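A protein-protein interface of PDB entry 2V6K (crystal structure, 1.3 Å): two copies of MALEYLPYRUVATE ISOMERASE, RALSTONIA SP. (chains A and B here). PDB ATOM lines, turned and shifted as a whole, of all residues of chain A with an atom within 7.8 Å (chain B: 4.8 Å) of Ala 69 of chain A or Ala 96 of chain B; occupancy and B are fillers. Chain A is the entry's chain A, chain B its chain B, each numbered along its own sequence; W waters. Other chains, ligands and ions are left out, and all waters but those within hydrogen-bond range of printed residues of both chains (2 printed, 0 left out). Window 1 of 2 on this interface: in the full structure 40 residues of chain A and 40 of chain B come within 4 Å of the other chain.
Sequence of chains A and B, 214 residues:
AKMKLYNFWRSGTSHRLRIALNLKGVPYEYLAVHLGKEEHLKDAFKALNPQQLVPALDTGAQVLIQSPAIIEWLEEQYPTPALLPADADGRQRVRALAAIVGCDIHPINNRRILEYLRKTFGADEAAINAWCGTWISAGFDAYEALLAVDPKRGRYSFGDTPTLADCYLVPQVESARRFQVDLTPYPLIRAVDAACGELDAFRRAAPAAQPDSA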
ATOM      1  N   ARG A  16     -10.271  18.360  -5.593  1.00  0.00           N
ATOM      2  CA  ARG A  16      -9.298  19.007  -4.715  1.00  0.00           C
ATOM      3  C   ARG A  16      -9.061  20.468  -5.110  1.00  0.00           C
ATOM      4  O   ARG A  16      -9.131  21.378  -4.274  1.00  0.00           O
ATOM      5  CB  ARG A  16      -7.999  18.196  -4.780  1.00  0.00           C
ATOM      6  CG  ARG A  16      -6.850  18.638  -3.885  1.00  0.00           C
ATOM      7  CD  ARG A  16      -5.557  18.005  -4.364  1.00  0.00           C
ATOM      8  NE  ARG A  16      -5.586  16.554  -4.200  1.00  0.00           N
ATOM      9  CZ  ARG A  16      -4.650  15.727  -4.657  1.00  0.00           C
ATOM     10  NH1 ARG A  16      -3.620  16.198  -5.355  1.00  0.00           N
ATOM     11  NH2 ARG A  16      -4.748  14.423  -4.426  1.00  0.00           N
ATOM     12  N   LEU A  17      -8.788  20.688  -6.390  1.00  0.00           N
ATOM     13  CA  LEU A  17      -8.519  22.033  -6.876  1.00  0.00           C
ATOM     14  C   LEU A  17      -9.782  22.897  -6.891  1.00  0.00           C
ATOM     15  O   LEU A  17      -9.723  24.093  -6.572  1.00  0.00           O
ATOM     16  CB  LEU A  17      -7.844  21.982  -8.249  1.00  0.00           C
ATOM     17  CG  LEU A  17      -7.528  23.323  -8.918  1.00  0.00           C
ATOM     18  CD1 LEU A  17      -6.749  24.252  -7.988  1.00  0.00           C
ATOM     19  CD2 LEU A  17      -6.749  23.090 -10.188  1.00  0.00           C
ATOM     20  N   GLN A  51       1.691  15.931 -19.686  1.00  0.00           N
ATOM     21  CA  GLN A  51       1.474  14.809 -18.792  1.00  0.00           C
ATOM     22  C   GLN A  51       0.123  14.114 -19.023  1.00  0.00           C
ATOM     23  O   GLN A  51      -0.071  12.973 -18.605  1.00  0.00           O
ATOM     24  CB  GLN A  51       1.604  15.274 -17.344  1.00  0.00           C
ATOM     25  CG  GLN A  51       1.949  14.144 -16.416  1.00  0.00           C
ATOM     26  CD  GLN A  51       2.094  14.559 -14.972  1.00  0.00           C
ATOM     27  OE1 GLN A  51       1.825  15.706 -14.588  1.00  0.00           O
ATOM     28  NE2 GLN A  51       2.514  13.610 -14.149  1.00  0.00           N
ATOM     29  N   LEU A  64      -1.058  25.957 -16.115  1.00  0.00           N
ATOM     30  CA  LEU A  64      -0.451  25.378 -14.930  1.00  0.00           C
ATOM     31  C   LEU A  64      -0.897  23.942 -14.770  1.00  0.00           C
ATOM     32  O   LEU A  64      -2.062  23.615 -15.017  1.00  0.00           O
ATOM     33  CB  LEU A  64      -0.867  26.156 -13.686  1.00  0.00           C
ATOM     34  CG  LEU A  64      -0.667  27.675 -13.673  1.00  0.00           C
ATOM     35  CD1 LEU A  64      -1.076  28.217 -12.329  1.00  0.00           C
ATOM     36  CD2 LEU A  64       0.766  28.063 -13.999  1.00  0.00           C
ATOM     37  N   ILE A  65       0.033  23.093 -14.355  1.00  0.00           N
ATOM     38  CA  ILE A  65      -0.284  21.702 -14.054  1.00  0.00           C
ATOM     39  C   ILE A  65       0.133  21.370 -12.626  1.00  0.00           C
ATOM     40  O   ILE A  65       0.811  22.167 -11.969  1.00  0.00           O
ATOM     41  CB  ILE A  65       0.366  20.714 -15.063  1.00  0.00           C
ATOM     42  CG1 ILE A  65       1.893  20.701 -14.922  1.00  0.00           C
ATOM     43  CG2 ILE A  65      -0.073  21.051 -16.488  1.00  0.00           C
ATOM     44  CD1 ILE A  65       2.562  19.493 -15.566  1.00  0.00           C
ATOM     45  N   GLN A  66      -0.278  20.187 -12.170  1.00  0.00           N
ATOM     46  CA  GLN A  66       0.016  19.658 -10.830  1.00  0.00           C
ATOM     47  C   GLN A  66      -0.782  20.342  -9.729  1.00  0.00           C
ATOM     48  O   GLN A  66      -0.396  21.407  -9.226  1.00  0.00           O
ATOM     49  CB  GLN A  66       1.515  19.674 -10.525  1.00  0.00           C
ATOM     50  CG  GLN A  66       2.246  18.576 -11.269  1.00  0.00           C
ATOM     51  CD  GLN A  66       1.844  17.190 -10.813  1.00  0.00           C
ATOM     52  OE1 GLN A  66       1.465  16.976  -9.653  1.00  0.00           O
ATOM     53  NE2 GLN A  66       1.909  16.229 -11.734  1.00  0.00           N
ATOM     54  N   SER A  67      -1.894  19.724  -9.337  1.00  0.00           N
ATOM     55  CA  SER A  67      -2.742  20.334  -8.317  1.00  0.00           C
ATOM     56  C   SER A  67      -1.992  20.776  -7.046  1.00  0.00           C
ATOM     57  O   SER A  67      -2.313  21.832  -6.515  1.00  0.00           O
ATOM     58  CB  SER A  67      -3.981  19.478  -8.006  1.00  0.00           C
ATOM     59  OG  SER A  67      -3.676  18.278  -7.324  1.00  0.00           O
ATOM     60  N   PRO A  68      -0.995  20.003  -6.552  1.00  0.00           N
ATOM     61  CA  PRO A  68      -0.327  20.527  -5.353  1.00  0.00           C
ATOM     62  C   PRO A  68       0.355  21.877  -5.575  1.00  0.00           C
ATOM     63  O   PRO A  68       0.295  22.757  -4.704  1.00  0.00           O
ATOM     64  CB  PRO A  68       0.703  19.440  -5.026  1.00  0.00           C
ATOM     65  CG  PRO A  68       0.085  18.202  -5.583  1.00  0.00           C
ATOM     66  CD  PRO A  68      -0.470  18.666  -6.898  1.00  0.00           C
ATOM     67  N   ALA A  69       0.994  22.028  -6.734  1.00  0.00           N
ATOM     68  CA  ALA A  69       1.683  23.265  -7.099  1.00  0.00           C
ATOM     69  C   ALA A  69       0.699  24.396  -7.400  1.00  0.00           C
ATOM     70  O   ALA A  69       0.929  25.555  -7.017  1.00  0.00           O
ATOM     71  CB  ALA A  69       2.588  23.017  -8.290  1.00  0.00           C
ATOM     72  N   ILE A  70      -0.388  24.068  -8.094  1.00  0.00           N
ATOM     73  CA  ILE A  70      -1.423  25.055  -8.382  1.00  0.00           C
ATOM     74  C   ILE A  70      -2.044  25.572  -7.090  1.00  0.00           C
ATOM     75  O   ILE A  70      -2.255  26.779  -6.946  1.00  0.00           O
ATOM     76  CB  ILE A  70      -2.523  24.486  -9.304  1.00  0.00           C
ATOM     77  CG1 ILE A  70      -1.926  24.071 -10.649  1.00  0.00           C
ATOM     78  CG2 ILE A  70      -3.630  25.523  -9.505  1.00  0.00           C
ATOM     79  CD1 ILE A  70      -2.861  23.239 -11.522  1.00  0.00           C
ATOM     80  N   ILE A  71      -2.338  24.677  -6.155  1.00  0.00           N
ATOM     81  CA  ILE A  71      -2.949  25.097  -4.893  1.00  0.00           C
ATOM     82  C   ILE A  71      -2.015  25.992  -4.071  1.00  0.00           C
ATOM     83  O   ILE A  71      -2.459  27.010  -3.520  1.00  0.00           O
ATOM     84  CB  ILE A  71      -3.486  23.894  -4.101  1.00  0.00           C
ATOM     85  CG1 ILE A  71      -4.656  23.268  -4.871  1.00  0.00           C
ATOM     86  CG2 ILE A  71      -3.923  24.318  -2.691  1.00  0.00           C
ATOM     87  CD1 ILE A  71      -5.108  21.914  -4.330  1.00  0.00           C
ATOM     88  N   GLU A  72      -0.724  25.653  -4.015  1.00  0.00           N
ATOM     89  CA  GLU A  72       0.263  26.527  -3.365  1.00  0.00           C
ATOM     90  C   GLU A  72       0.333  27.900  -4.045  1.00  0.00           C
ATOM     91  O   GLU A  72       0.462  28.931  -3.371  1.00  0.00           O
ATOM     92  CB  GLU A  72       1.643  25.871  -3.357  1.00  0.00           C
ATOM     93  CG  GLU A  72       1.754  24.627  -2.486  1.00  0.00           C
ATOM     94  CD  GLU A  72       2.275  24.894  -1.082  1.00  0.00           C
ATOM     95  OE1 GLU A  72       2.488  26.068  -0.701  1.00  0.00           O
ATOM     96  OE2 GLU A  72       2.504  23.901  -0.360  1.00  0.00           O
ATOM     97  N   TRP A  73       0.235  27.910  -5.374  1.00  0.00           N
ATOM     98  CA  TRP A  73       0.196  29.152  -6.151  1.00  0.00           C
ATOM     99  C   TRP A  73      -1.041  29.990  -5.808  1.00  0.00           C
ATOM    100  O   TRP A  73      -0.932  31.200  -5.589  1.00  0.00           O
ATOM    101  CB  TRP A  73       0.292  28.819  -7.645  1.00  0.00           C
ATOM    102  CG  TRP A  73       0.185  29.967  -8.607  1.00  0.00           C
ATOM    103  CD1 TRP A  73       1.198  30.765  -9.054  1.00  0.00           C
ATOM    104  CD2 TRP A  73      -1.002  30.417  -9.270  1.00  0.00           C
ATOM    105  NE1 TRP A  73       0.712  31.695  -9.945  1.00  0.00           N
ATOM    106  CE2 TRP A  73      -0.637  31.499 -10.095  1.00  0.00           C
ATOM    107  CE3 TRP A  73      -2.344  30.005  -9.243  1.00  0.00           C
ATOM    108  CZ2 TRP A  73      -1.566  32.188 -10.884  1.00  0.00           C
ATOM    109  CZ3 TRP A  73      -3.268  30.691 -10.028  1.00  0.00           C
ATOM    110  CH2 TRP A  73      -2.871  31.765 -10.835  1.00  0.00           C
ATOM    111  N   LEU A  74      -2.208  29.348  -5.732  1.00  0.00           N
ATOM    112  CA  LEU A  74      -3.437  30.041  -5.330  1.00  0.00           C
ATOM    113  C   LEU A  74      -3.311  30.670  -3.955  1.00  0.00           C
ATOM    114  O   LEU A  74      -3.766  31.795  -3.745  1.00  0.00           O
ATOM    115  CB  LEU A  74      -4.631  29.087  -5.321  1.00  0.00           C
ATOM    116  CG  LEU A  74      -5.179  28.627  -6.664  1.00  0.00           C
ATOM    117  CD1 LEU A  74      -6.253  27.584  -6.431  1.00  0.00           C
ATOM    118  CD2 LEU A  74      -5.762  29.808  -7.432  1.00  0.00           C
ATOM    119  N   GLU A  75      -2.703  29.951  -3.015  1.00  0.00           N
ATOM    120  CA  GLU A  75      -2.553  30.456  -1.655  1.00  0.00           C
ATOM    121  C   GLU A  75      -1.744  31.752  -1.631  1.00  0.00           C
ATOM    122  O   GLU A  75      -2.079  32.685  -0.897  1.00  0.00           O
ATOM    123  CB  GLU A  75      -1.913  29.387  -0.758  1.00  0.00           C
ATOM    124  CG  GLU A  75      -1.488  29.882   0.619  1.00  0.00           C
ATOM    125  CD  GLU A  75      -2.640  30.332   1.505  1.00  0.00           C
ATOM    126  OE1 GLU A  75      -3.825  30.177   1.128  1.00  0.00           O
ATOM    127  OE2 GLU A  75      -2.341  30.840   2.601  1.00  0.00           O
ATOM    128  N   TYR A 168      -7.499  18.287   0.159  1.00  0.00           N
ATOM    129  CA  TYR A 168      -7.051  16.951  -0.227  1.00  0.00           C
ATOM    130  C   TYR A 168      -7.895  15.856   0.420  1.00  0.00           C
ATOM    131  O   TYR A 168      -8.198  14.844  -0.217  1.00  0.00           O
ATOM    132  CB  TYR A 168      -5.600  16.729   0.184  1.00  0.00           C
ATOM    133  CG  TYR A 168      -4.529  17.427  -0.628  1.00  0.00           C
ATOM    134  CD1 TYR A 168      -3.594  16.683  -1.353  1.00  0.00           C
ATOM    135  CD2 TYR A 168      -4.389  18.816  -0.611  1.00  0.00           C
ATOM    136  CE1 TYR A 168      -2.574  17.299  -2.059  1.00  0.00           C
ATOM    137  CE2 TYR A 168      -3.362  19.446  -1.318  1.00  0.00           C
ATOM    138  CZ  TYR A 168      -2.454  18.677  -2.031  1.00  0.00           C
ATOM    139  OH  TYR A 168      -1.418  19.269  -2.703  1.00  0.00           O
ATOM    140  N   GLN B  92       5.781  28.003  -8.797  1.00  0.00           N
ATOM    141  CA  GLN B  92       4.799  27.031  -9.255  1.00  0.00           C
ATOM    142  C   GLN B  92       5.434  25.991 -10.177  1.00  0.00           C
ATOM    143  O   GLN B  92       5.141  24.795 -10.054  1.00  0.00           O
ATOM    144  CB  GLN B  92       3.619  27.737  -9.921  1.00  0.00           C
ATOM    145  CG  GLN B  92       2.366  26.871 -10.059  1.00  0.00           C
ATOM    146  CD  GLN B  92       2.440  25.885 -11.208  1.00  0.00           C
ATOM    147  OE1 GLN B  92       3.174  26.088 -12.182  1.00  0.00           O
ATOM    148  NE2 GLN B  92       1.663  24.812 -11.108  1.00  0.00           N
ATOM    149  N   ARG B  93       6.309  26.431 -11.078  1.00  0.00           N
ATOM    150  CA  ARG B  93       6.954  25.520 -12.032  1.00  0.00           C
ATOM    151  C   ARG B  93       7.866  24.519 -11.342  1.00  0.00           C
ATOM    152  O   ARG B  93       7.870  23.338 -11.691  1.00  0.00           O
ATOM    153  CB  ARG B  93       7.774  26.284 -13.078  1.00  0.00           C
ATOM    154  CG  ARG B  93       7.038  27.376 -13.823  1.00  0.00           C
ATOM    155  CD  ARG B  93       5.909  26.838 -14.671  1.00  0.00           C
ATOM    156  NE  ARG B  93       5.102  27.942 -15.184  1.00  0.00           N
ATOM    157  CZ  ARG B  93       3.991  27.813 -15.903  1.00  0.00           C
ATOM    158  NH1 ARG B  93       3.514  26.614 -16.223  1.00  0.00           N
ATOM    159  NH2 ARG B  93       3.351  28.903 -16.297  1.00  0.00           N
ATOM    160  N   VAL B  94       8.648  24.992 -10.377  1.00  0.00           N
ATOM    161  CA  VAL B  94       9.549  24.117  -9.628  1.00  0.00           C
ATOM    162  C   VAL B  94       8.736  23.127  -8.795  1.00  0.00           C
ATOM    163  O   VAL B  94       9.044  21.932  -8.764  1.00  0.00           O
ATOM    164  CB  VAL B  94      10.541  24.927  -8.763  1.00  0.00           C
ATOM    165  CG1 VAL B  94      11.334  24.003  -7.854  1.00  0.00           C
ATOM    166  CG2 VAL B  94      11.493  25.706  -9.655  1.00  0.00           C
ATOM    167  N   ARG B  95       7.681  23.606  -8.142  1.00  0.00           N
ATOM    168  CA  ARG B  95       6.807  22.700  -7.403  1.00  0.00           C
ATOM    169  C   ARG B  95       6.123  21.679  -8.309  1.00  0.00           C
ATOM    170  O   ARG B  95       5.925  20.538  -7.897  1.00  0.00           O
ATOM    171  CB  ARG B  95       5.775  23.479  -6.590  1.00  0.00           C
ATOM    172  CG  ARG B  95       6.355  24.170  -5.370  1.00  0.00           C
ATOM    173  CD  ARG B  95       5.240  24.759  -4.527  1.00  0.00           C
ATOM    174  NE  ARG B  95       5.730  25.310  -3.265  1.00  0.00           N
ATOM    175  CZ  ARG B  95       5.580  26.566  -2.870  1.00  0.00           C
ATOM    176  NH1 ARG B  95       4.938  27.449  -3.629  1.00  0.00           N
ATOM    177  NH2 ARG B  95       6.068  26.932  -1.698  1.00  0.00           N
ATOM    178  N   ALA B  96       5.776  22.082  -9.531  1.00  0.00           N
ATOM    179  CA  ALA B  96       5.123  21.168 -10.467  1.00  0.00           C
ATOM    180  C   ALA B  96       6.079  20.065 -10.907  1.00  0.00           C
ATOM    181  O   ALA B  96       5.700  18.892 -10.929  1.00  0.00           O
ATOM    182  CB  ALA B  96       4.568  21.919 -11.669  1.00  0.00           C
ATOM    183  N   LEU B  97       7.314  20.427 -11.242  1.00  0.00           N
ATOM    184  CA  LEU B  97       8.319  19.424 -11.594  1.00  0.00           C
ATOM    185  C   LEU B  97       8.518  18.438 -10.457  1.00  0.00           C
ATOM    186  O   LEU B  97       8.525  17.224 -10.681  1.00  0.00           O
ATOM    187  CB  LEU B  97       9.652  20.087 -11.943  1.00  0.00           C
ATOM    188  CG  LEU B  97       9.702  20.845 -13.272  1.00  0.00           C
ATOM    189  CD1 LEU B  97      10.979  21.662 -13.357  1.00  0.00           C
ATOM    190  CD2 LEU B  97       9.583  19.909 -14.476  1.00  0.00           C
ATOM    191  N   ALA B  98       8.668  18.951  -9.236  1.00  0.00           N
ATOM    192  CA  ALA B  98       8.844  18.085  -8.076  1.00  0.00           C
ATOM    193  C   ALA B  98       7.656  17.147  -7.926  1.00  0.00           C
ATOM    194  O   ALA B  98       7.841  15.960  -7.652  1.00  0.00           O
ATOM    195  CB  ALA B  98       9.037  18.919  -6.816  1.00  0.00           C
ATOM    196  N   ALA B  99       6.444  17.674  -8.095  1.00  0.00           N
ATOM    197  CA  ALA B  99       5.238  16.881  -7.867  1.00  0.00           C
ATOM    198  C   ALA B  99       5.024  15.799  -8.921  1.00  0.00           C
ATOM    199  O   ALA B  99       4.455  14.759  -8.613  1.00  0.00           O
ATOM    200  CB  ALA B  99       4.011  17.785  -7.744  1.00  0.00           C
ATOM    201  N   ILE B 100       5.496  16.021 -10.146  1.00  0.00           N
ATOM    202  CA  ILE B 100       5.462  14.939 -11.140  1.00  0.00           C
ATOM    203  C   ILE B 100       6.159  13.714 -10.550  1.00  0.00           C
ATOM    204  O   ILE B 100       5.627  12.599 -10.580  1.00  0.00           O
ATOM    205  CB  ILE B 100       6.136  15.350 -12.465  1.00  0.00           C
ATOM    206  CG1 ILE B 100       5.271  16.384 -13.190  1.00  0.00           C
ATOM    207  CG2 ILE B 100       6.398  14.118 -13.352  1.00  0.00           C
ATOM    208  CD1 ILE B 100       5.927  16.993 -14.417  1.00  0.00           C
HETATM  209  O   HOH W   1       3.436  27.085  -6.168  1.00  0.00           O
HETATM  210  O   HOH W   2       2.695  24.197 -14.099  1.00  0.00           O
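Ile 100 of chain B touches Gln 51 of chain A. OE1 of Gln 92 of chain B touches CD2 of Leu 64 of chain A, 3.6 Å away. Arg 93 of chain B touches Leu 64 of chain A. O of Ile 65 of chain A touches CB of Ala 96 of chain B (3.8 Å). Ala 96 of chain B touches Gln 66 of chain A (O to CG, 3.5 Å). Ala 99 of chain B touches Gln 66 of chain A (CB to OE1, 3.3 Å). NE2 of Gln 66 of chain A touches CG1 of Ile 100 of chain B, 3.7 Å away. Gln 92 of chain B touches Ala 69 of chain A. CG1 of Ile 70 of chain A touches NE2 of Gln 92 of chain B, 3.7 Å away. CG of Gln 92 of chain B touches CB of Trp 73 of chain A (3.7 Å).
Of the 9 printed residues of chain B, 6 touch a printed residue of chain A. Printed residues of chain B that touch a printed residue of chain A: Gln 92, Arg 93, Arg 95, Ala 96, Ala 99 and Ile 100. Along chain A the printed residues that touch a printed residue of chain B span positions 51 to 73. Among the printed residues, 14 pairs touch across the chains. Among the printed residues, Asp or Glu carboxylates within 4 Å of a Lys or Arg side-chain nitrogen of the other chain: Glu 72 of chain A with Arg 95 of chain B (3.8 Å).
NH2 of Arg 95 of chain B is in salt-bridge range of OE1 of Glu 72 of chain A, 3.8 Å away. The backbone carbonyl oxygen of Ile 65 of chain A lies within hydrogen-bond range of the side-chain amide nitrogen of Gln 92 of chain B.
The side-chain amide nitrogen (NE2) of Gln 66 of chain A is in hydrogen-bond range of the side-chain amide oxygen (OE1) of Gln 51 of chain A (2.9 Å).
Printed residues of chain B within 4 Å of Leu 64 of chain A: Gln 92 (3.6 Å) and Arg 93 (3.6 Å). Printed residues of chain B within 4 Å of Gln 66 of chain A: Ala 96 (3.5 Å), Ala 99 (3.3 Å) and Ile 100 (3.7 Å). Of chain B, only Gln 92, Arg 95 and Ala 96 come within 4 Å of Ala 69 of chain A. Tyr 168 of chain A touches none of the printed residues of chain B. Of the printed residues of chain A, Arg 95 of chain B touches Ala 69 and Glu 72. Ala 96 of chain B touches just these residues of chain A: Ile 65 (3.8 Å), Gln 66 (3.5 Å) and Ala 69 (3.5 Å). Printed residues of chain A within 4 Å of Ile 100 of chain B: Gln 51 and Gln 66. The nearest printed residue of chain B that does not touch Ala 69 of chain A is Ala 99 of chain B (5.3 Å).
No position is printed for both chains. Of the 14 pairs that touch across the chains among the printed residues, none has its exchanged pair printed and touching as well.
Water W2 lies within hydrogen-bond range of OE1 of Gln 92 of chain B, N of Ile 65 of chain A and NH1 of Arg 93 of chain B. Water W1 lies within hydrogen-bond range of the guanidinium group of Arg 95 of chain B (3.0 Å), the backbone carbonyl oxygen of Ala 69 of chain A (3.1 Å) and the backbone NH of Trp 73 of chain A (3.4 Å).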
